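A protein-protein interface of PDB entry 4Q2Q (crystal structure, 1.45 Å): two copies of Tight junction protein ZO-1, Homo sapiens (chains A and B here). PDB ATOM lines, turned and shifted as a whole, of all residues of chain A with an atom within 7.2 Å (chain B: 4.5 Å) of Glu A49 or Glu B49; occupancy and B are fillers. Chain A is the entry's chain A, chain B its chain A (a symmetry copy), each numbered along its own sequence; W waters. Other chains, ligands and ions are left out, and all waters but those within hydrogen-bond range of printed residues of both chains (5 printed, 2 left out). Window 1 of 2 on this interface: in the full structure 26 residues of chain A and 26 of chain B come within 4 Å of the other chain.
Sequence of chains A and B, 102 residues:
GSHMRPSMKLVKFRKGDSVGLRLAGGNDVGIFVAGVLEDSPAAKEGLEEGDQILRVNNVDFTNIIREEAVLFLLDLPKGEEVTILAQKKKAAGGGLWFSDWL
The guanidinium group (NH1) of Arg A22 is in salt-bridge range of the side-chain carboxylate (OE1) of Glu B49 (3.7 Å).
The side-chain carboxylate (OE2) of Glu B49 sits close to the backbone carbonyl oxygen (O) of Ala A34 (2.6 Å).
OE1 of Glu A49 lies within salt-bridge range of NH1 of Arg B22, 3.7 Å away.
O of Ala B34 sits close to OE2 of Glu A49 (2.6 Å).
O of Ser A99 sits at hydrogen-bond distance from NH2 of Arg B22 (3.1 Å).
The backbone carbonyl oxygen (O) of Arg A22 is in hydrogen-bond range of the backbone NH (N) of Ala A34.
O of Gly A35 lies within hydrogen-bond range of N of Arg A22, 3.0 Å away.
The backbone carbonyl oxygen (O) of Ala A24 sits at hydrogen-bond distance from the backbone NH (N) of Phe A32, 2.8 Å away.
The backbone NH of Ala B34 lies within hydrogen-bond range of the backbone carbonyl oxygen of Arg B22 (2.8 Å).
The backbone NH of Arg B22 sits at hydrogen-bond distance from the backbone carbonyl oxygen of Gly B35 (3.0 Å).
Among the printed residues, merely in contact across the chains: Leu A23 with Phe B98, Ala A24 with Phe B98, Ala A34 with Ala B34, Glu A49 with Glu B49, Trp A101 with Arg B22, Trp A101 with Gly B35 and Trp A101 with Val B36.
Val A36 touches none of the printed residues of chain B.
Of the printed residues of chain B, Glu A49 touches Arg B22, Ala B34 and Glu B49.
Of the printed residues of chain A, Gly B35 touches Trp A101.
Printed residues of chain A within 4 Å of Val B36: Trp A101.
Gly B50 touches none of the printed residues of chain A.
The nearest printed residue of chain A that does not touch Glu B49 is Gly A35 (4.6 Å).
Of the 18 printed residues of chain A, 7 touch a printed residue of chain B.
Printed residues of chain A that touch a printed residue of chain B: Arg A22, Leu A23, Ala A24, Ala A34, Glu A49, Ser A99 and Trp A101.
Hydrophobic or aromatic side chains of chain A within 4 Å of the printed part of chain B: Ala A24, Ala A34 and Trp A101.
Of the 10 printed residues of chain B, 6 touch a printed residue of chain A.
Hydrophobic or aromatic side chains of chain B within 4 Å of the printed part of chain A: Ala B34 and Phe B98.
Among the printed residues, Asp or Glu carboxylates within 4 Å of a Lys or Arg side-chain nitrogen of the other chain: Arg A22 with Glu B49 (3.7 Å) and Glu A49 with Arg B22 (3.7 Å).
Arg A22 touches Glu B49, and with the chains exchanged Glu A49 touches Arg B22.
Ala B34 touches its own counterpart, Ala A34.
Ala A34 touches Glu B49, and with the chains exchanged Glu A49 touches Ala B34.
Glu A49 touches its own counterpart, Glu B49.
Positions printed for both chains: 22, 33, 34, 35, 36, 48, 49, 50, 51 and 98.
Of the 12 pairs that touch across the chains among the printed residues, 6 have their exchanged pair printed and touching as well.
Water W5 lies within hydrogen-bond range of the backbone carbonyl oxygen of Glu A49 (2.7 Å) and the guanidinium group of Arg B22 (3.1 Å).
Water W2 lies within hydrogen-bond range of O of Glu B49 and NH2 of Arg A22.
Water W4 lies within hydrogen-bond range of O of Ser A99 and NE of Arg B22.
Water W3 bridges NH1 of Arg A22 (2.7 Å) and OE1 of Glu B49 (3.1 Å).
Water W1 bridges the guanidinium group of Arg B22 (2.7 Å) and the side-chain carboxylate of Glu A49 (3.1 Å).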
ATOM      1  N   ARG A  22       2.967 -28.099  -6.287  1.00  0.00           N
ATOM      2  CA  ARG A  22       1.671 -28.424  -5.738  1.00  0.00           C
ATOM      3  C   ARG A  22       0.664 -27.495  -6.389  1.00  0.00           C
ATOM      4  O   ARG A  22       1.018 -26.388  -6.828  1.00  0.00           O
ATOM      5  CB  ARG A  22       1.647 -28.395  -4.203  1.00  0.00           C
ATOM      6  CG  ARG A  22       2.079 -27.143  -3.552  1.00  0.00           C
ATOM      7  CD  ARG A  22       2.299 -27.370  -2.036  1.00  0.00           C
ATOM      8  NE  ARG A  22       1.207 -28.122  -1.454  1.00  0.00           N
ATOM      9  CZ  ARG A  22       1.146 -28.521  -0.182  1.00  0.00           C
ATOM     10  NH1 ARG A  22       2.158 -28.267   0.677  1.00  0.00           N
ATOM     11  NH2 ARG A  22       0.092 -29.233   0.211  1.00  0.00           N
ATOM     12  N   LEU A  23      -0.595 -27.940  -6.442  1.00  0.00           N
ATOM     13  CA  LEU A  23      -1.680 -27.257  -7.160  1.00  0.00           C
ATOM     14  C   LEU A  23      -2.775 -26.791  -6.199  1.00  0.00           C
ATOM     15  O   LEU A  23      -2.987 -27.365  -5.124  1.00  0.00           O
ATOM     16  CB  LEU A  23      -2.330 -28.205  -8.183  1.00  0.00           C
ATOM     17  CG  LEU A  23      -1.459 -28.781  -9.284  1.00  0.00           C
ATOM     18  CD1 LEU A  23      -2.259 -29.698 -10.176  1.00  0.00           C
ATOM     19  CD2 LEU A  23      -0.754 -27.703 -10.061  1.00  0.00           C
ATOM     20  N   ALA A  24      -3.503 -25.773  -6.648  1.00  0.00           N
ATOM     21  CA  ALA A  24      -4.725 -25.335  -5.968  1.00  0.00           C
ATOM     22  C   ALA A  24      -5.740 -24.912  -7.009  1.00  0.00           C
ATOM     23  O   ALA A  24      -5.406 -24.472  -8.109  1.00  0.00           O
ATOM     24  CB  ALA A  24      -4.451 -24.175  -4.944  1.00  0.00           C
ATOM     25  N   PHE A  32      -3.966 -23.548 -10.371  1.00  0.00           N
ATOM     26  CA  PHE A  32      -2.913 -22.598  -9.957  1.00  0.00           C
ATOM     27  C   PHE A  32      -1.735 -23.317  -9.297  1.00  0.00           C
ATOM     28  O   PHE A  32      -1.930 -24.373  -8.676  1.00  0.00           O
ATOM     29  CB  PHE A  32      -3.478 -21.565  -8.980  1.00  0.00           C
ATOM     30  CG  PHE A  32      -4.507 -20.663  -9.622  1.00  0.00           C
ATOM     31  CD1 PHE A  32      -5.824 -21.117  -9.850  1.00  0.00           C
ATOM     32  CD2 PHE A  32      -4.158 -19.416 -10.089  1.00  0.00           C
ATOM     33  CE1 PHE A  32      -6.733 -20.320 -10.483  1.00  0.00           C
ATOM     34  CE2 PHE A  32      -5.097 -18.627 -10.716  1.00  0.00           C
ATOM     35  CZ  PHE A  32      -6.364 -19.103 -10.926  1.00  0.00           C
ATOM     36  N   VAL A  33      -0.539 -22.730  -9.435  1.00  0.00           N
ATOM     37  CA  VAL A  33       0.631 -23.169  -8.691  1.00  0.00           C
ATOM     38  C   VAL A  33       0.497 -22.746  -7.222  1.00  0.00           C
ATOM     39  O   VAL A  33       0.395 -21.571  -6.926  1.00  0.00           O
ATOM     40  CB  VAL A  33       1.914 -22.597  -9.283  1.00  0.00           C
ATOM     41  CG1 VAL A  33       3.127 -23.084  -8.470  1.00  0.00           C
ATOM     42  CG2 VAL A  33       2.042 -22.996 -10.760  1.00  0.00           C
ATOM     43  N   ALA A  34       0.436 -23.728  -6.323  1.00  0.00           N
ATOM     44  CA  ALA A  34       0.308 -23.478  -4.890  1.00  0.00           C
ATOM     45  C   ALA A  34       1.630 -23.700  -4.144  1.00  0.00           C
ATOM     46  O   ALA A  34       1.680 -23.581  -2.924  1.00  0.00           O
ATOM     47  CB  ALA A  34      -0.801 -24.372  -4.284  1.00  0.00           C
ATOM     48  N   GLY A  35       2.696 -23.969  -4.858  1.00  0.00           N
ATOM     49  CA  GLY A  35       3.977 -24.190  -4.232  1.00  0.00           C
ATOM     50  C   GLY A  35       4.939 -24.747  -5.263  1.00  0.00           C
ATOM     51  O   GLY A  35       4.528 -25.490  -6.169  1.00  0.00           O
ATOM     52  N   VAL A  36       6.209 -24.341  -5.143  1.00  0.00           N
ATOM     53  CA  VAL A  36       7.298 -24.827  -6.001  1.00  0.00           C
ATOM     54  C   VAL A  36       8.416 -25.318  -5.088  1.00  0.00           C
ATOM     55  O   VAL A  36       8.819 -24.643  -4.178  1.00  0.00           O
ATOM     56  CB  VAL A  36       7.802 -23.742  -6.968  1.00  0.00           C
ATOM     57  CG1 VAL A  36       8.837 -24.294  -7.917  1.00  0.00           C
ATOM     58  CG2 VAL A  36       6.614 -23.133  -7.757  1.00  0.00           C
ATOM     59  N   GLY A  46      11.864 -20.952 -12.967  1.00  0.00           N
ATOM     60  CA  GLY A  46      11.058 -19.752 -12.716  1.00  0.00           C
ATOM     61  C   GLY A  46       9.572 -19.930 -12.478  1.00  0.00           C
ATOM     62  O   GLY A  46       8.860 -18.955 -12.550  1.00  0.00           O
ATOM     63  N   LEU A  47       9.083 -21.141 -12.216  1.00  0.00           N
ATOM     64  CA  LEU A  47       7.672 -21.311 -11.828  1.00  0.00           C
ATOM     65  C   LEU A  47       7.477 -20.649 -10.465  1.00  0.00           C
ATOM     66  O   LEU A  47       8.394 -20.718  -9.631  1.00  0.00           O
ATOM     67  CB  LEU A  47       7.314 -22.798 -11.810  1.00  0.00           C
ATOM     68  CG  LEU A  47       5.838 -23.184 -11.782  1.00  0.00           C
ATOM     69  CD1 LEU A  47       5.157 -22.776 -13.098  1.00  0.00           C
ATOM     70  CD2 LEU A  47       5.667 -24.647 -11.543  1.00  0.00           C
ATOM     71  N   GLU A  48       6.338 -19.964 -10.252  1.00  0.00           N
ATOM     72  CA  GLU A  48       6.048 -19.271  -8.973  1.00  0.00           C
ATOM     73  C   GLU A  48       4.655 -19.520  -8.443  1.00  0.00           C
ATOM     74  O   GLU A  48       3.716 -19.671  -9.214  1.00  0.00           O
ATOM     75  CB  GLU A  48       6.243 -17.782  -9.109  1.00  0.00           C
ATOM     76  CG  GLU A  48       7.695 -17.432  -9.425  1.00  0.00           C
ATOM     77  CD  GLU A  48       7.933 -15.949  -9.607  1.00  0.00           C
ATOM     78  OE1 GLU A  48       6.938 -15.184  -9.681  1.00  0.00           O
ATOM     79  OE2 GLU A  48       9.127 -15.556  -9.661  1.00  0.00           O
ATOM     80  N   GLU A  49       4.530 -19.589  -7.116  1.00  0.00           N
ATOM     81  CA  GLU A  49       3.236 -19.736  -6.448  1.00  0.00           C
ATOM     82  C   GLU A  49       2.357 -18.574  -6.903  1.00  0.00           C
ATOM     83  O   GLU A  49       2.820 -17.428  -6.996  1.00  0.00           O
ATOM     84  CB  GLU A  49       3.404 -19.773  -4.923  1.00  0.00           C
ATOM     85  CG  GLU A  49       2.088 -19.885  -4.179  1.00  0.00           C
ATOM     86  CD  GLU A  49       2.115 -20.521  -2.815  1.00  0.00           C
ATOM     87  OE1 GLU A  49       3.189 -20.939  -2.335  1.00  0.00           O
ATOM     88  OE2 GLU A  49       0.995 -20.605  -2.218  1.00  0.00           O
ATOM     89  N   GLY A  50       1.097 -18.884  -7.221  1.00  0.00           N
ATOM     90  CA  GLY A  50       0.124 -17.888  -7.682  1.00  0.00           C
ATOM     91  C   GLY A  50      -0.089 -17.830  -9.169  1.00  0.00           C
ATOM     92  O   GLY A  50      -1.090 -17.301  -9.638  1.00  0.00           O
ATOM     93  N   ASP A  51       0.859 -18.398  -9.916  1.00  0.00           N
ATOM     94  CA  ASP A  51       0.744 -18.498 -11.373  1.00  0.00           C
ATOM     95  C   ASP A  51      -0.466 -19.388 -11.729  1.00  0.00           C
ATOM     96  O   ASP A  51      -0.671 -20.414 -11.107  1.00  0.00           O
ATOM     97  CB  ASP A  51       2.022 -19.151 -11.969  1.00  0.00           C
ATOM     98  CG  ASP A  51       3.237 -18.252 -11.935  1.00  0.00           C
ATOM     99  OD1 ASP A  51       3.060 -17.034 -11.647  1.00  0.00           O
ATOM    100  OD2 ASP A  51       4.357 -18.790 -12.241  1.00  0.00           O
ATOM    101  N   GLN A  52      -1.243 -19.030 -12.747  1.00  0.00           N
ATOM    102  CA  GLN A  52      -2.247 -19.944 -13.274  1.00  0.00           C
ATOM    103  C   GLN A  52      -1.573 -20.790 -14.356  1.00  0.00           C
ATOM    104  O   GLN A  52      -0.907 -20.263 -15.248  1.00  0.00           O
ATOM    105  CB  GLN A  52      -3.424 -19.184 -13.881  1.00  0.00           C
ATOM    106  CG  GLN A  52      -4.575 -20.157 -14.276  1.00  0.00           C
ATOM    107  CD  GLN A  52      -5.758 -19.523 -14.942  1.00  0.00           C
ATOM    108  OE1 GLN A  52      -5.899 -18.293 -14.974  1.00  0.00           O
ATOM    109  NE2 GLN A  52      -6.624 -20.364 -15.506  1.00  0.00           N
ATOM    110  N   PHE A  98      -3.630 -15.056  -4.417  1.00  0.00           N
ATOM    111  CA  PHE A  98      -2.580 -15.477  -3.510  1.00  0.00           C
ATOM    112  C   PHE A  98      -1.849 -14.241  -2.980  1.00  0.00           C
ATOM    113  O   PHE A  98      -1.416 -13.377  -3.762  1.00  0.00           O
ATOM    114  CB  PHE A  98      -1.542 -16.344  -4.260  1.00  0.00           C
ATOM    115  CG  PHE A  98      -2.053 -17.721  -4.642  1.00  0.00           C
ATOM    116  CD1 PHE A  98      -2.895 -17.890  -5.715  1.00  0.00           C
ATOM    117  CD2 PHE A  98      -1.651 -18.848  -3.928  1.00  0.00           C
ATOM    118  CE1 PHE A  98      -3.362 -19.150  -6.046  1.00  0.00           C
ATOM    119  CE2 PHE A  98      -2.112 -20.121  -4.263  1.00  0.00           C
ATOM    120  CZ  PHE A  98      -2.941 -20.258  -5.328  1.00  0.00           C
ATOM    121  N   SER A  99      -1.688 -14.166  -1.671  1.00  0.00           N
ATOM    122  CA  SER A  99      -0.929 -13.080  -1.061  1.00  0.00           C
ATOM    123  C   SER A  99       0.550 -13.358  -1.167  1.00  0.00           C
ATOM    124  O   SER A  99       0.959 -14.465  -1.474  1.00  0.00           O
ATOM    125  CB  SER A  99      -1.302 -12.892   0.415  1.00  0.00           C
ATOM    126  OG  SER A  99      -0.679 -13.859   1.233  1.00  0.00           O
ATOM    127  N   TRP A 101       4.149 -13.469   1.160  1.00  0.00           N
ATOM    128  CA  TRP A 101       4.483 -13.820   2.525  1.00  0.00           C
ATOM    129  C   TRP A 101       4.156 -12.650   3.455  1.00  0.00           C
ATOM    130  O   TRP A 101       4.500 -11.499   3.162  1.00  0.00           O
ATOM    131  CB  TRP A 101       5.963 -14.150   2.641  1.00  0.00           C
ATOM    132  CG  TRP A 101       6.341 -15.513   2.071  1.00  0.00           C
ATOM    133  CD1 TRP A 101       7.072 -15.758   0.957  1.00  0.00           C
ATOM    134  CD2 TRP A 101       5.956 -16.788   2.580  1.00  0.00           C
ATOM    135  NE1 TRP A 101       7.220 -17.107   0.761  1.00  0.00           N
ATOM    136  CE2 TRP A 101       6.535 -17.768   1.739  1.00  0.00           C
ATOM    137  CE3 TRP A 101       5.181 -17.206   3.658  1.00  0.00           C
ATOM    138  CZ2 TRP A 101       6.350 -19.130   1.946  1.00  0.00           C
ATOM    139  CZ3 TRP A 101       5.006 -18.563   3.867  1.00  0.00           C
ATOM    140  CH2 TRP A 101       5.593 -19.514   3.009  1.00  0.00           C
ATOM    141  N   ARG B  22       1.445 -17.383   4.081  1.00  0.00           N
ATOM    142  CA  ARG B  22       0.856 -16.742   2.929  1.00  0.00           C
ATOM    143  C   ARG B  22      -0.562 -17.264   2.804  1.00  0.00           C
ATOM    144  O   ARG B  22      -0.867 -18.380   3.260  1.00  0.00           O
ATOM    145  CB  ARG B  22       1.697 -16.908   1.656  1.00  0.00           C
ATOM    146  CG  ARG B  22       2.028 -18.287   1.248  1.00  0.00           C
ATOM    147  CD  ARG B  22       3.122 -18.280   0.153  1.00  0.00           C
ATOM    148  NE  ARG B  22       2.834 -17.298  -0.870  1.00  0.00           N
ATOM    149  CZ  ARG B  22       3.626 -17.021  -1.909  1.00  0.00           C
ATOM    150  NH1 ARG B  22       4.815 -17.643  -2.064  1.00  0.00           N
ATOM    151  NH2 ARG B  22       3.249 -16.069  -2.759  1.00  0.00           N
ATOM    152  N   VAL B  33      -4.625 -21.147   4.166  1.00  0.00           N
ATOM    153  CA  VAL B  33      -3.173 -21.147   4.261  1.00  0.00           C
ATOM    154  C   VAL B  33      -2.571 -21.649   2.942  1.00  0.00           C
ATOM    155  O   VAL B  33      -2.830 -22.763   2.530  1.00  0.00           O
ATOM    156  CB  VAL B  33      -2.692 -22.015   5.417  1.00  0.00           C
ATOM    157  CG1 VAL B  33      -1.154 -21.989   5.483  1.00  0.00           C
ATOM    158  CG2 VAL B  33      -3.311 -21.534   6.737  1.00  0.00           C
ATOM    159  N   ALA B  34      -1.818 -20.783   2.263  1.00  0.00           N
ATOM    160  CA  ALA B  34      -1.179 -21.119   0.994  1.00  0.00           C
ATOM    161  C   ALA B  34       0.326 -21.370   1.153  1.00  0.00           C
ATOM    162  O   ALA B  34       1.020 -21.614   0.171  1.00  0.00           O
ATOM    163  CB  ALA B  34      -1.424 -19.998  -0.045  1.00  0.00           C
ATOM    164  N   GLY B  35       0.822 -21.363   2.367  1.00  0.00           N
ATOM    165  CA  GLY B  35       2.227 -21.592   2.600  1.00  0.00           C
ATOM    166  C   GLY B  35       2.548 -21.251   4.041  1.00  0.00           C
ATOM    167  O   GLY B  35       1.940 -20.336   4.622  1.00  0.00           O
ATOM    168  N   VAL B  36       3.473 -22.024   4.623  1.00  0.00           N
ATOM    169  CA  VAL B  36       3.969 -21.803   5.988  1.00  0.00           C
ATOM    170  C   VAL B  36       5.492 -21.755   5.920  1.00  0.00           C
ATOM    171  O   VAL B  36       6.116 -22.602   5.339  1.00  0.00           O
ATOM    172  CB  VAL B  36       3.488 -22.892   6.963  1.00  0.00           C
ATOM    173  CG1 VAL B  36       3.910 -22.584   8.378  1.00  0.00           C
ATOM    174  CG2 VAL B  36       1.947 -23.044   6.879  1.00  0.00           C
ATOM    175  N   GLU B  48      -0.617 -25.737   8.466  1.00  0.00           N
ATOM    176  CA  GLU B  48      -0.322 -26.431   7.188  1.00  0.00           C
ATOM    177  C   GLU B  48      -1.020 -25.831   5.988  1.00  0.00           C
ATOM    178  O   GLU B  48      -2.134 -25.336   6.103  1.00  0.00           O
ATOM    179  CB  GLU B  48      -0.691 -27.891   7.268  1.00  0.00           C
ATOM    180  CG  GLU B  48       0.144 -28.624   8.316  1.00  0.00           C
ATOM    181  CD  GLU B  48      -0.216 -30.087   8.459  1.00  0.00           C
ATOM    182  OE1 GLU B  48      -1.250 -30.511   7.883  1.00  0.00           O
ATOM    183  OE2 GLU B  48       0.556 -30.809   9.141  1.00  0.00           O
ATOM    184  N   GLU B  49      -0.344 -25.855   4.838  1.00  0.00           N
ATOM    185  CA  GLU B  49      -0.918 -25.395   3.572  1.00  0.00           C
ATOM    186  C   GLU B  49      -2.196 -26.195   3.337  1.00  0.00           C
ATOM    187  O   GLU B  49      -2.233 -27.413   3.567  1.00  0.00           O
ATOM    188  CB  GLU B  49       0.085 -25.554   2.422  1.00  0.00           C
ATOM    189  CG  GLU B  49      -0.472 -25.129   1.079  1.00  0.00           C
ATOM    190  CD  GLU B  49       0.509 -24.661   0.038  1.00  0.00           C
ATOM    191  OE1 GLU B  49       1.731 -24.628   0.292  1.00  0.00           O
ATOM    192  OE2 GLU B  49       0.010 -24.306  -1.078  1.00  0.00           O
ATOM    193  N   GLY B  50      -3.254 -25.497   2.914  1.00  0.00           N
ATOM    194  CA  GLY B  50      -4.559 -26.111   2.646  1.00  0.00           C
ATOM    195  C   GLY B  50      -5.581 -25.962   3.738  1.00  0.00           C
ATOM    196  O   GLY B  50      -6.774 -26.123   3.505  1.00  0.00           O
ATOM    197  N   ASP B  51      -5.106 -25.633   4.940  1.00  0.00           N
ATOM    198  CA  ASP B  51      -5.990 -25.365   6.077  1.00  0.00           C
ATOM    199  C   ASP B  51      -6.858 -24.127   5.769  1.00  0.00           C
ATOM    200  O   ASP B  51      -6.360 -23.150   5.241  1.00  0.00           O
ATOM    201  CB  ASP B  51      -5.150 -25.067   7.351  1.00  0.00           C
ATOM    202  CG  ASP B  51      -4.462 -26.285   7.925  1.00  0.00           C
ATOM    203  OD1 ASP B  51      -4.797 -27.418   7.474  1.00  0.00           O
ATOM    204  OD2 ASP B  51      -3.615 -26.077   8.861  1.00  0.00           O
ATOM    205  N   PHE B  98      -6.438 -27.999  -2.421  1.00  0.00           N
ATOM    206  CA  PHE B  98      -4.991 -27.996  -2.529  1.00  0.00           C
ATOM    207  C   PHE B  98      -4.496 -29.438  -2.667  1.00  0.00           C
ATOM    208  O   PHE B  98      -4.862 -30.313  -1.863  1.00  0.00           O
ATOM    209  CB  PHE B  98      -4.360 -27.409  -1.246  1.00  0.00           C
ATOM    210  CG  PHE B  98      -4.562 -25.913  -1.091  1.00  0.00           C
ATOM    211  CD1 PHE B  98      -5.767 -25.400  -0.673  1.00  0.00           C
ATOM    212  CD2 PHE B  98      -3.514 -25.029  -1.342  1.00  0.00           C
ATOM    213  CE1 PHE B  98      -5.939 -24.033  -0.547  1.00  0.00           C
ATOM    214  CE2 PHE B  98      -3.682 -23.651  -1.207  1.00  0.00           C
ATOM    215  CZ  PHE B  98      -4.881 -23.174  -0.791  1.00  0.00           C
HETATM  216  O   HOH W   1       5.984 -19.963  -1.386  1.00  0.00           O
HETATM  217  O   HOH W   2      -0.517 -29.433   3.242  1.00  0.00           O
HETATM  218  O   HOH W   3       4.129 -26.474   1.004  1.00  0.00           O
HETATM  219  O   HOH W   4      -0.077 -16.942  -1.435  1.00  0.00           O
HETATM  220  O   HOH W   5       4.555 -15.986  -5.567  1.00  0.00           O
